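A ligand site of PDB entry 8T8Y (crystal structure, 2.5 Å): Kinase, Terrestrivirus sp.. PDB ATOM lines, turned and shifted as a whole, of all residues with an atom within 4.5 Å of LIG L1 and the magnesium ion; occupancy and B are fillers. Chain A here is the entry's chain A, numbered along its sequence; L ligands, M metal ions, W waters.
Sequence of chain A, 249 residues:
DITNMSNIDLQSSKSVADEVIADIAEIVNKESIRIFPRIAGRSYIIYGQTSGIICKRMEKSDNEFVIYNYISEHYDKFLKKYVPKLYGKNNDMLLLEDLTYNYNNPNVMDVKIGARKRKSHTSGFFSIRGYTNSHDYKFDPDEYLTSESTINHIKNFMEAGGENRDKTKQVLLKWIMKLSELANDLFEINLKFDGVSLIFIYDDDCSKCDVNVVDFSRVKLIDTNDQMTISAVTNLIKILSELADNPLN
The side-chain amino group of Lys 56 is in salt-bridge range of the side-chain carboxylate of Asp 215. O of Ser 43 sits close to NH1 of Arg 38, 3.5 Å away. The side-chain carboxylate (OD1) of Asp 110 is in hydrogen-bond range of the side-chain hydroxyl (OG) of Ser 197. The backbone carbonyl oxygen (O) of Gly 41 is in hydrogen-bond range of the guanidinium group (NH2) of Arg 38. The backbone carbonyl oxygen (O) of Ala 40 sits at hydrogen-bond distance from the guanidinium group (NE) of Arg 38 (3.1 Å). The backbone carbonyl oxygen (O) of Ile 54 lies within hydrogen-bond range of the backbone NH (N) of Leu 96, 2.7 Å away. The backbone carbonyl oxygen (O) of Ile 45 sits at hydrogen-bond distance from the backbone NH (N) of Phe 36, 3.0 Å away. OG1 of Thr 100 sits at hydrogen-bond distance from OD1 of Asp 98 (2.6 Å).
Of the 23 residues printed, 1 comes within 4 Å of the magnesium ion. The nearest printed residue that does not touch the magnesium ion is Lys 112 (4.2 Å).
The magnesium ion is bound by water W4 (2.0 Å), an oxygen (O10) of LG2 L2 (2.1 Å), the side-chain carboxylate of Asp 215 (2.1 Å), an oxygen (O4) of LIG L1 (2.1 Å), water W3 (2.2 Å) and an oxygen (O1) of LIG L1 (2.3 Å). The magnesium ion has six donor atoms within binding distance.
Merely in contact with LIG L1: Phe 36, Arg 38, Ala 40, Gly 41, Ile 45, Ile 54, Pro 84 and Asp 98. Hydrophobic or aromatic side chains within 4 Å of LIG L1: Phe 36, Ile 39, Ala 40, Ile 45, Ile 54, Pro 84 and Leu 99. The nearest printed residue that does not touch LIG L1 is Ile 199 (4.01 Å).
Water W4 lies within hydrogen-bond range of OG of Ser 197 (2.7 Å) and NZ of Lys 112 (3.3 Å). Water W2 lies within hydrogen-bond range of O3 of LG2 L2, O3 of LIG L1 and OD1 of Asp 215.
The backbone NH of Ser 43 lies within hydrogen-bond range of an oxygen (O2) of LIG L1, 2.8 Å away. The side-chain hydroxyl of Ser 43 lies within hydrogen-bond range of an oxygen (O3) of LIG L1 (2.5 Å). OD2 of Asp 110 is in hydrogen-bond range of O9 of LIG L1 (2.7 Å). The backbone carbonyl oxygen (O) of Glu 97 sits at hydrogen-bond distance from a nitrogen (N3) of LIG L1 (2.8 Å). O5 of LIG L1 lies within salt-bridge range of NZ of Lys 56 (2.8 Å). N of Arg 42 sits at hydrogen-bond distance from O2 of LIG L1, 2.9 Å away. The backbone NH (N) of Leu 99 is in hydrogen-bond range of a nitrogen (N4) of LIG L1 (2.9 Å). The backbone NH (N) of Ile 39 is in hydrogen-bond range of an oxygen (O10) of LIG L1 (3.2 Å). The guanidinium group (NE) of Arg 42 is in salt-bridge range of an oxygen (O11) of LG2 L2 (3.0 Å). The side-chain amino group (NZ) of Lys 112 is in salt-bridge range of an oxygen (O13) of LG2 L2 (2.4 Å).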
ATOM      1  N   PHE A  36       0.120 -17.885  15.411  1.00  0.00           N
ATOM      2  CA  PHE A  36      -1.131 -17.302  14.845  1.00  0.00           C
ATOM      3  C   PHE A  36      -1.011 -15.784  14.884  1.00  0.00           C
ATOM      4  O   PHE A  36      -0.581 -15.236  15.901  1.00  0.00           O
ATOM      5  CB  PHE A  36      -2.378 -17.773  15.595  1.00  0.00           C
ATOM      6  CG  PHE A  36      -3.644 -17.324  14.931  1.00  0.00           C
ATOM      7  CD1 PHE A  36      -4.159 -18.037  13.849  1.00  0.00           C
ATOM      8  CD2 PHE A  36      -4.280 -16.153  15.315  1.00  0.00           C
ATOM      9  CE1 PHE A  36      -5.317 -17.611  13.215  1.00  0.00           C
ATOM     10  CE2 PHE A  36      -5.438 -15.726  14.671  1.00  0.00           C
ATOM     11  CZ  PHE A  36      -5.947 -16.458  13.626  1.00  0.00           C
ATOM     12  N   ARG A  38      -2.279 -13.076  15.914  1.00  0.00           N
ATOM     13  CA  ARG A  38      -3.047 -12.289  16.912  1.00  0.00           C
ATOM     14  C   ARG A  38      -3.035 -10.809  16.492  1.00  0.00           C
ATOM     15  O   ARG A  38      -2.009 -10.325  15.960  1.00  0.00           O
ATOM     16  CB  ARG A  38      -2.422 -12.413  18.307  1.00  0.00           C
ATOM     17  CG  ARG A  38      -2.843 -13.651  19.095  1.00  0.00           C
ATOM     18  CD  ARG A  38      -2.126 -13.737  20.439  1.00  0.00           C
ATOM     19  NE  ARG A  38      -1.749 -12.402  20.850  1.00  0.00           N
ATOM     20  CZ  ARG A  38      -0.509 -11.962  21.051  1.00  0.00           C
ATOM     21  NH1 ARG A  38       0.546 -12.757  20.928  1.00  0.00           N
ATOM     22  NH2 ARG A  38      -0.315 -10.692  21.392  1.00  0.00           N
ATOM     23  N   ILE A  39      -4.143 -10.107  16.728  1.00  0.00           N
ATOM     24  CA  ILE A  39      -4.285  -8.668  16.396  1.00  0.00           C
ATOM     25  C   ILE A  39      -4.330  -7.853  17.691  1.00  0.00           C
ATOM     26  O   ILE A  39      -4.323  -6.609  17.613  1.00  0.00           O
ATOM     27  CB  ILE A  39      -5.493  -8.503  15.446  1.00  0.00           C
ATOM     28  CG1 ILE A  39      -5.075  -7.700  14.209  1.00  0.00           C
ATOM     29  CG2 ILE A  39      -6.732  -7.931  16.131  1.00  0.00           C
ATOM     30  CD1 ILE A  39      -4.041  -8.419  13.366  1.00  0.00           C
ATOM     31  N   ALA A  40      -4.306  -8.541  18.834  1.00  0.00           N
ATOM     32  CA  ALA A  40      -4.377  -7.952  20.186  1.00  0.00           C
ATOM     33  C   ALA A  40      -4.140  -9.051  21.218  1.00  0.00           C
ATOM     34  O   ALA A  40      -3.901 -10.199  20.814  1.00  0.00           O
ATOM     35  CB  ALA A  40      -5.722  -7.285  20.376  1.00  0.00           C
ATOM     36  N   GLY A  41      -4.185  -8.720  22.512  1.00  0.00           N
ATOM     37  CA  GLY A  41      -3.955  -9.691  23.599  1.00  0.00           C
ATOM     38  C   GLY A  41      -2.490 -10.062  23.725  1.00  0.00           C
ATOM     39  O   GLY A  41      -1.646  -9.281  23.253  1.00  0.00           O
ATOM     40  N   ARG A  42      -2.198 -11.210  24.352  1.00  0.00           N
ATOM     41  CA  ARG A  42      -0.819 -11.608  24.724  1.00  0.00           C
ATOM     42  C   ARG A  42      -0.652 -13.138  24.795  1.00  0.00           C
ATOM     43  O   ARG A  42       0.506 -13.581  24.885  1.00  0.00           O
ATOM     44  CB  ARG A  42      -0.467 -10.980  26.069  1.00  0.00           C
ATOM     45  CG  ARG A  42      -1.323 -11.477  27.236  1.00  0.00           C
ATOM     46  CD  ARG A  42      -1.630 -10.378  28.239  1.00  0.00           C
ATOM     47  NE  ARG A  42      -2.351  -9.293  27.584  1.00  0.00           N
ATOM     48  CZ  ARG A  42      -1.867  -8.070  27.316  1.00  0.00           C
ATOM     49  NH1 ARG A  42      -0.633  -7.744  27.668  1.00  0.00           N
ATOM     50  NH2 ARG A  42      -2.628  -7.183  26.703  1.00  0.00           N
ATOM     51  N   SER A  43      -1.738 -13.916  24.769  1.00  0.00           N
ATOM     52  CA  SER A  43      -1.721 -15.391  24.916  1.00  0.00           C
ATOM     53  C   SER A  43      -0.906 -16.028  23.796  1.00  0.00           C
ATOM     54  O   SER A  43      -0.823 -15.449  22.687  1.00  0.00           O
ATOM     55  CB  SER A  43      -3.116 -15.965  24.959  1.00  0.00           C
ATOM     56  OG  SER A  43      -3.694 -15.782  26.256  1.00  0.00           O
ATOM     57  N   ILE A  45      -0.890 -18.260  21.048  1.00  0.00           N
ATOM     58  CA  ILE A  45      -1.898 -18.809  20.101  1.00  0.00           C
ATOM     59  C   ILE A  45      -1.158 -19.208  18.830  1.00  0.00           C
ATOM     60  O   ILE A  45      -0.434 -18.368  18.273  1.00  0.00           O
ATOM     61  CB  ILE A  45      -3.044 -17.826  19.819  1.00  0.00           C
ATOM     62  CG1 ILE A  45      -3.674 -17.323  21.114  1.00  0.00           C
ATOM     63  CG2 ILE A  45      -4.069 -18.483  18.902  1.00  0.00           C
ATOM     64  CD1 ILE A  45      -4.933 -16.507  20.918  1.00  0.00           C
ATOM     65  N   ILE A  54      -7.258 -23.099  15.642  1.00  0.00           N
ATOM     66  CA  ILE A  54      -6.177 -22.419  16.423  1.00  0.00           C
ATOM     67  C   ILE A  54      -6.122 -23.037  17.815  1.00  0.00           C
ATOM     68  O   ILE A  54      -7.188 -23.438  18.351  1.00  0.00           O
ATOM     69  CB  ILE A  54      -6.385 -20.892  16.472  1.00  0.00           C
ATOM     70  CG1 ILE A  54      -7.703 -20.506  17.139  1.00  0.00           C
ATOM     71  CG2 ILE A  54      -6.252 -20.308  15.071  1.00  0.00           C
ATOM     72  CD1 ILE A  54      -7.637 -19.191  17.891  1.00  0.00           C
ATOM     73  N   LYS A  56      -5.044 -22.229  21.686  1.00  0.00           N
ATOM     74  CA  LYS A  56      -4.813 -21.124  22.649  1.00  0.00           C
ATOM     75  C   LYS A  56      -4.316 -21.709  23.982  1.00  0.00           C
ATOM     76  O   LYS A  56      -5.033 -22.522  24.554  1.00  0.00           O
ATOM     77  CB  LYS A  56      -6.077 -20.304  22.861  1.00  0.00           C
ATOM     78  CG  LYS A  56      -5.928 -19.164  23.858  1.00  0.00           C
ATOM     79  CD  LYS A  56      -7.183 -18.349  24.079  1.00  0.00           C
ATOM     80  CE  LYS A  56      -7.029 -17.478  25.311  1.00  0.00           C
ATOM     81  NZ  LYS A  56      -8.190 -16.577  25.511  1.00  0.00           N
ATOM     82  N   PRO A  84     -16.906 -18.845  19.113  1.00  0.00           N
ATOM     83  CA  PRO A  84     -16.243 -19.849  18.284  1.00  0.00           C
ATOM     84  C   PRO A  84     -16.360 -21.226  18.954  1.00  0.00           C
ATOM     85  O   PRO A  84     -16.241 -21.302  20.177  1.00  0.00           O
ATOM     86  CB  PRO A  84     -14.776 -19.398  18.241  1.00  0.00           C
ATOM     87  CG  PRO A  84     -14.630 -18.477  19.441  1.00  0.00           C
ATOM     88  CD  PRO A  84     -15.986 -17.810  19.589  1.00  0.00           C
ATOM     89  N   LEU A  96      -9.641 -24.268  19.192  1.00  0.00           N
ATOM     90  CA  LEU A  96     -10.759 -23.339  18.880  1.00  0.00           C
ATOM     91  C   LEU A  96     -10.923 -23.223  17.358  1.00  0.00           C
ATOM     92  O   LEU A  96      -9.906 -23.289  16.639  1.00  0.00           O
ATOM     93  CB  LEU A  96     -10.474 -21.967  19.488  1.00  0.00           C
ATOM     94  CG  LEU A  96     -10.536 -21.877  21.011  1.00  0.00           C
ATOM     95  CD1 LEU A  96     -10.183 -20.476  21.495  1.00  0.00           C
ATOM     96  CD2 LEU A  96     -11.896 -22.294  21.533  1.00  0.00           C
ATOM     97  N   GLU A  97     -12.166 -23.056  16.916  1.00  0.00           N
ATOM     98  CA  GLU A  97     -12.504 -22.579  15.548  1.00  0.00           C
ATOM     99  C   GLU A  97     -11.697 -21.305  15.240  1.00  0.00           C
ATOM    100  O   GLU A  97     -11.757 -20.366  16.038  1.00  0.00           O
ATOM    101  CB  GLU A  97     -13.993 -22.305  15.464  1.00  0.00           C
ATOM    102  CG  GLU A  97     -14.446 -21.752  14.126  1.00  0.00           C
ATOM    103  CD  GLU A  97     -15.883 -21.239  14.151  1.00  0.00           C
ATOM    104  OE1 GLU A  97     -16.569 -21.426  15.180  1.00  0.00           O
ATOM    105  OE2 GLU A  97     -16.303 -20.654  13.136  1.00  0.00           O
ATOM    106  N   ASP A  98     -10.966 -21.302  14.126  1.00  0.00           N
ATOM    107  CA  ASP A  98     -10.302 -20.093  13.587  1.00  0.00           C
ATOM    108  C   ASP A  98     -11.354 -19.249  12.884  1.00  0.00           C
ATOM    109  O   ASP A  98     -11.788 -19.645  11.794  1.00  0.00           O
ATOM    110  CB  ASP A  98      -9.163 -20.436  12.626  1.00  0.00           C
ATOM    111  CG  ASP A  98      -8.496 -19.213  12.018  1.00  0.00           C
ATOM    112  OD1 ASP A  98      -8.923 -18.070  12.323  1.00  0.00           O
ATOM    113  OD2 ASP A  98      -7.565 -19.409  11.221  1.00  0.00           O
ATOM    114  N   LEU A  99     -11.753 -18.132  13.490  1.00  0.00           N
ATOM    115  CA  LEU A  99     -12.797 -17.221  12.963  1.00  0.00           C
ATOM    116  C   LEU A  99     -12.349 -16.539  11.663  1.00  0.00           C
ATOM    117  O   LEU A  99     -13.208 -15.952  10.990  1.00  0.00           O
ATOM    118  CB  LEU A  99     -13.128 -16.182  14.035  1.00  0.00           C
ATOM    119  CG  LEU A  99     -13.769 -16.734  15.302  1.00  0.00           C
ATOM    120  CD1 LEU A  99     -13.767 -15.683  16.409  1.00  0.00           C
ATOM    121  CD2 LEU A  99     -15.187 -17.217  15.025  1.00  0.00           C
ATOM    122  N   THR A 100     -11.063 -16.580  11.316  1.00  0.00           N
ATOM    123  CA  THR A 100     -10.538 -15.961  10.068  1.00  0.00           C
ATOM    124  C   THR A 100     -10.496 -16.998   8.944  1.00  0.00           C
ATOM    125  O   THR A 100     -10.217 -16.581   7.812  1.00  0.00           O
ATOM    126  CB  THR A 100      -9.143 -15.360  10.264  1.00  0.00           C
ATOM    127  OG1 THR A 100      -8.216 -16.424  10.442  1.00  0.00           O
ATOM    128  CG2 THR A 100      -9.074 -14.416  11.445  1.00  0.00           C
ATOM    129  N   VAL A 108      -9.511  -7.939  10.923  1.00  0.00           N
ATOM    130  CA  VAL A 108      -9.938  -8.304  12.294  1.00  0.00           C
ATOM    131  C   VAL A 108      -9.789  -7.073  13.207  1.00  0.00           C
ATOM    132  O   VAL A 108      -8.736  -6.424  13.125  1.00  0.00           O
ATOM    133  CB  VAL A 108      -9.094  -9.469  12.826  1.00  0.00           C
ATOM    134  CG1 VAL A 108      -9.607  -9.964  14.170  1.00  0.00           C
ATOM    135  CG2 VAL A 108      -9.014 -10.601  11.809  1.00  0.00           C
ATOM    136  N   ASP A 110     -10.341  -6.445  17.503  1.00  0.00           N
ATOM    137  CA  ASP A 110     -10.646  -6.895  18.883  1.00  0.00           C
ATOM    138  C   ASP A 110     -11.159  -5.665  19.649  1.00  0.00           C
ATOM    139  O   ASP A 110     -10.384  -4.698  19.761  1.00  0.00           O
ATOM    140  CB  ASP A 110      -9.400  -7.501  19.517  1.00  0.00           C
ATOM    141  CG  ASP A 110      -9.598  -8.098  20.913  1.00  0.00           C
ATOM    142  OD1 ASP A 110     -10.384  -7.494  21.692  1.00  0.00           O
ATOM    143  OD2 ASP A 110      -8.922  -9.143  21.218  1.00  0.00           O
ATOM    144  N   LYS A 112     -12.787  -4.779  23.415  1.00  0.00           N
ATOM    145  CA  LYS A 112     -13.027  -5.258  24.803  1.00  0.00           C
ATOM    146  C   LYS A 112     -14.342  -4.648  25.288  1.00  0.00           C
ATOM    147  O   LYS A 112     -14.418  -3.414  25.368  1.00  0.00           O
ATOM    148  CB  LYS A 112     -11.825  -4.831  25.641  1.00  0.00           C
ATOM    149  CG  LYS A 112     -11.836  -5.186  27.112  1.00  0.00           C
ATOM    150  CD  LYS A 112     -11.409  -6.599  27.367  1.00  0.00           C
ATOM    151  CE  LYS A 112      -9.913  -6.804  27.414  1.00  0.00           C
ATOM    152  NZ  LYS A 112      -9.584  -8.056  28.145  1.00  0.00           N
ATOM    153  N   SER A 197     -13.998  -9.980  24.630  1.00  0.00           N
ATOM    154  CA  SER A 197     -13.834  -9.122  23.445  1.00  0.00           C
ATOM    155  C   SER A 197     -14.807  -9.567  22.346  1.00  0.00           C
ATOM    156  O   SER A 197     -15.132 -10.755  22.291  1.00  0.00           O
ATOM    157  CB  SER A 197     -12.408  -9.131  22.966  1.00  0.00           C
ATOM    158  OG  SER A 197     -11.567  -8.427  23.885  1.00  0.00           O
ATOM    159  N   ILE A 199     -14.737  -9.877  18.398  1.00  0.00           N
ATOM    160  CA  ILE A 199     -13.819  -9.987  17.239  1.00  0.00           C
ATOM    161  C   ILE A 199     -14.629  -9.705  15.980  1.00  0.00           C
ATOM    162  O   ILE A 199     -15.372 -10.615  15.544  1.00  0.00           O
ATOM    163  CB  ILE A 199     -13.142 -11.375  17.203  1.00  0.00           C
ATOM    164  CG1 ILE A 199     -12.382 -11.652  18.503  1.00  0.00           C
ATOM    165  CG2 ILE A 199     -12.229 -11.504  15.990  1.00  0.00           C
ATOM    166  CD1 ILE A 199     -11.476 -10.510  18.937  1.00  0.00           C
ATOM    167  N   VAL A 214     -15.027 -13.664  22.392  1.00  0.00           N
ATOM    168  CA  VAL A 214     -13.869 -14.522  22.770  1.00  0.00           C
ATOM    169  C   VAL A 214     -13.298 -14.042  24.105  1.00  0.00           C
ATOM    170  O   VAL A 214     -13.691 -12.937  24.556  1.00  0.00           O
ATOM    171  CB  VAL A 214     -12.787 -14.517  21.670  1.00  0.00           C
ATOM    172  CG1 VAL A 214     -13.353 -14.933  20.327  1.00  0.00           C
ATOM    173  CG2 VAL A 214     -12.084 -13.175  21.575  1.00  0.00           C
ATOM    174  N   ASP A 215     -12.381 -14.844  24.668  1.00  0.00           N
ATOM    175  CA  ASP A 215     -11.617 -14.619  25.921  1.00  0.00           C
ATOM    176  C   ASP A 215     -12.558 -14.723  27.130  1.00  0.00           C
ATOM    177  O   ASP A 215     -13.011 -13.690  27.646  1.00  0.00           O
ATOM    178  CB  ASP A 215     -10.844 -13.290  25.908  1.00  0.00           C
ATOM    179  CG  ASP A 215      -9.706 -13.206  26.913  1.00  0.00           C
ATOM    180  OD1 ASP A 215      -9.619 -14.118  27.781  1.00  0.00           O
ATOM    181  OD2 ASP A 215      -8.891 -12.232  26.833  1.00  0.00           O
HETATM  182  P1  LIG L   1      -5.631 -13.167  25.095  1.00  0.00           P
HETATM  183  O1  LIG L   1      -6.284 -11.818  25.399  1.00  0.00           O
HETATM  184  O2  LIG L   1      -4.380 -13.042  24.278  1.00  0.00           O
HETATM  185  O3  LIG L   1      -5.439 -14.008  26.316  1.00  0.00           O
HETATM  186  P2  LIG L   1      -7.979 -13.630  23.290  1.00  0.00           P
HETATM  187  O4  LIG L   1      -8.471 -12.256  23.625  1.00  0.00           O
HETATM  188  O5  LIG L   1      -8.920 -14.776  23.444  1.00  0.00           O
HETATM  189  O6  LIG L   1      -6.679 -13.994  24.165  1.00  0.00           O
HETATM  190  O7  LIG L   1      -7.367 -13.628  21.805  1.00  0.00           O
HETATM  191  C1  LIG L   1      -6.477 -12.552  21.432  1.00  0.00           C
HETATM  192  C2  LIG L   1      -6.457 -12.404  19.933  1.00  0.00           C
HETATM  193  O8  LIG L   1      -6.425 -13.705  19.299  1.00  0.00           O
HETATM  194  C3  LIG L   1      -7.663 -11.684  19.312  1.00  0.00           C
HETATM  195  O9  LIG L   1      -7.408 -10.280  19.325  1.00  0.00           O
HETATM  196  C4  LIG L   1      -7.731 -12.289  17.901  1.00  0.00           C
HETATM  197  O10 LIG L   1      -6.937 -11.601  16.961  1.00  0.00           O
HETATM  198  C5  LIG L   1      -7.182 -13.703  18.110  1.00  0.00           C
HETATM  199  N1  LIG L   1      -8.207 -14.736  18.282  1.00  0.00           N
HETATM  200  C6  LIG L   1      -8.623 -15.286  19.466  1.00  0.00           C
HETATM  201  N2  LIG L   1      -9.525 -16.223  19.315  1.00  0.00           N
HETATM  202  C7  LIG L   1      -9.688 -16.315  17.937  1.00  0.00           C
HETATM  203  C8  LIG L   1     -10.499 -17.147  17.147  1.00  0.00           C
HETATM  204  N3  LIG L   1     -11.299 -18.079  17.632  1.00  0.00           N
HETATM  205  N4  LIG L   1     -10.404 -16.997  15.804  1.00  0.00           N
HETATM  206  C9  LIG L   1      -9.574 -16.070  15.308  1.00  0.00           C
HETATM  207  N5  LIG L   1      -8.774 -15.230  15.967  1.00  0.00           N
HETATM  208  C10 LIG L   1      -8.876 -15.407  17.294  1.00  0.00           C
HETATM  209  C1  LG2 L   2      -4.904  -9.299  32.634  1.00  0.00           C
HETATM  210  C2  LG2 L   2      -4.317 -10.223  31.552  1.00  0.00           C
HETATM  211  C3  LG2 L   2      -5.323 -10.393  30.443  1.00  0.00           C
HETATM  212  C4  LG2 L   2      -5.667  -9.042  29.812  1.00  0.00           C
HETATM  213  C5  LG2 L   2      -6.303  -8.147  30.887  1.00  0.00           C
HETATM  214  C6  LG2 L   2      -5.268  -7.949  32.032  1.00  0.00           C
HETATM  215  O1  LG2 L   2      -3.999  -9.080  33.738  1.00  0.00           O
HETATM  216  O2  LG2 L   2      -3.096  -9.661  31.011  1.00  0.00           O
HETATM  217  O3  LG2 L   2      -4.780 -11.293  29.456  1.00  0.00           O
HETATM  218  O4  LG2 L   2      -6.602  -9.259  28.738  1.00  0.00           O
HETATM  219  O5  LG2 L   2      -6.706  -6.871  30.290  1.00  0.00           O
HETATM  220  O6  LG2 L   2      -5.818  -7.158  33.100  1.00  0.00           O
HETATM  221  P1  LG2 L   2      -3.396 -10.277  34.683  1.00  0.00           P
HETATM  222  O7  LG2 L   2      -4.699 -11.029  35.021  1.00  0.00           O
HETATM  223  O8  LG2 L   2      -2.409 -11.015  33.682  1.00  0.00           O
HETATM  224  O9  LG2 L   2      -2.668  -9.663  35.825  1.00  0.00           O
HETATM  225  P2  LG2 L   2      -6.168  -9.106  27.204  1.00  0.00           P
HETATM  226  O10 LG2 L   2      -7.551  -9.397  26.497  1.00  0.00           O
HETATM  227  O11 LG2 L   2      -5.096 -10.233  26.988  1.00  0.00           O
HETATM  228  O12 LG2 L   2      -5.680  -7.714  27.030  1.00  0.00           O
HETATM  229  P3  LG2 L   2      -8.081  -6.087  30.664  1.00  0.00           P
HETATM  230  O13 LG2 L   2      -9.141  -7.194  30.363  1.00  0.00           O
HETATM  231  O14 LG2 L   2      -7.832  -4.942  29.618  1.00  0.00           O
HETATM  232  O15 LG2 L   2      -7.790  -5.823  32.070  1.00  0.00           O
HETATM  233 MG    MG M   1      -8.350 -10.892  25.275  1.00  0.00          MG
HETATM  234  O   HOH W   1     -10.088 -16.935  21.970  1.00  0.00           O
HETATM  235  O   HOH W   2      -6.761 -12.666  28.673  1.00  0.00           O
HETATM  236  O   HOH W   3      -7.854  -9.248  23.886  1.00  0.00           O
HETATM  237  O   HOH W   4     -10.116  -9.938  25.515  1.00  0.00           O
HETATM  238  O   HOH W   5      -7.570 -13.042  14.677  1.00  0.00           O
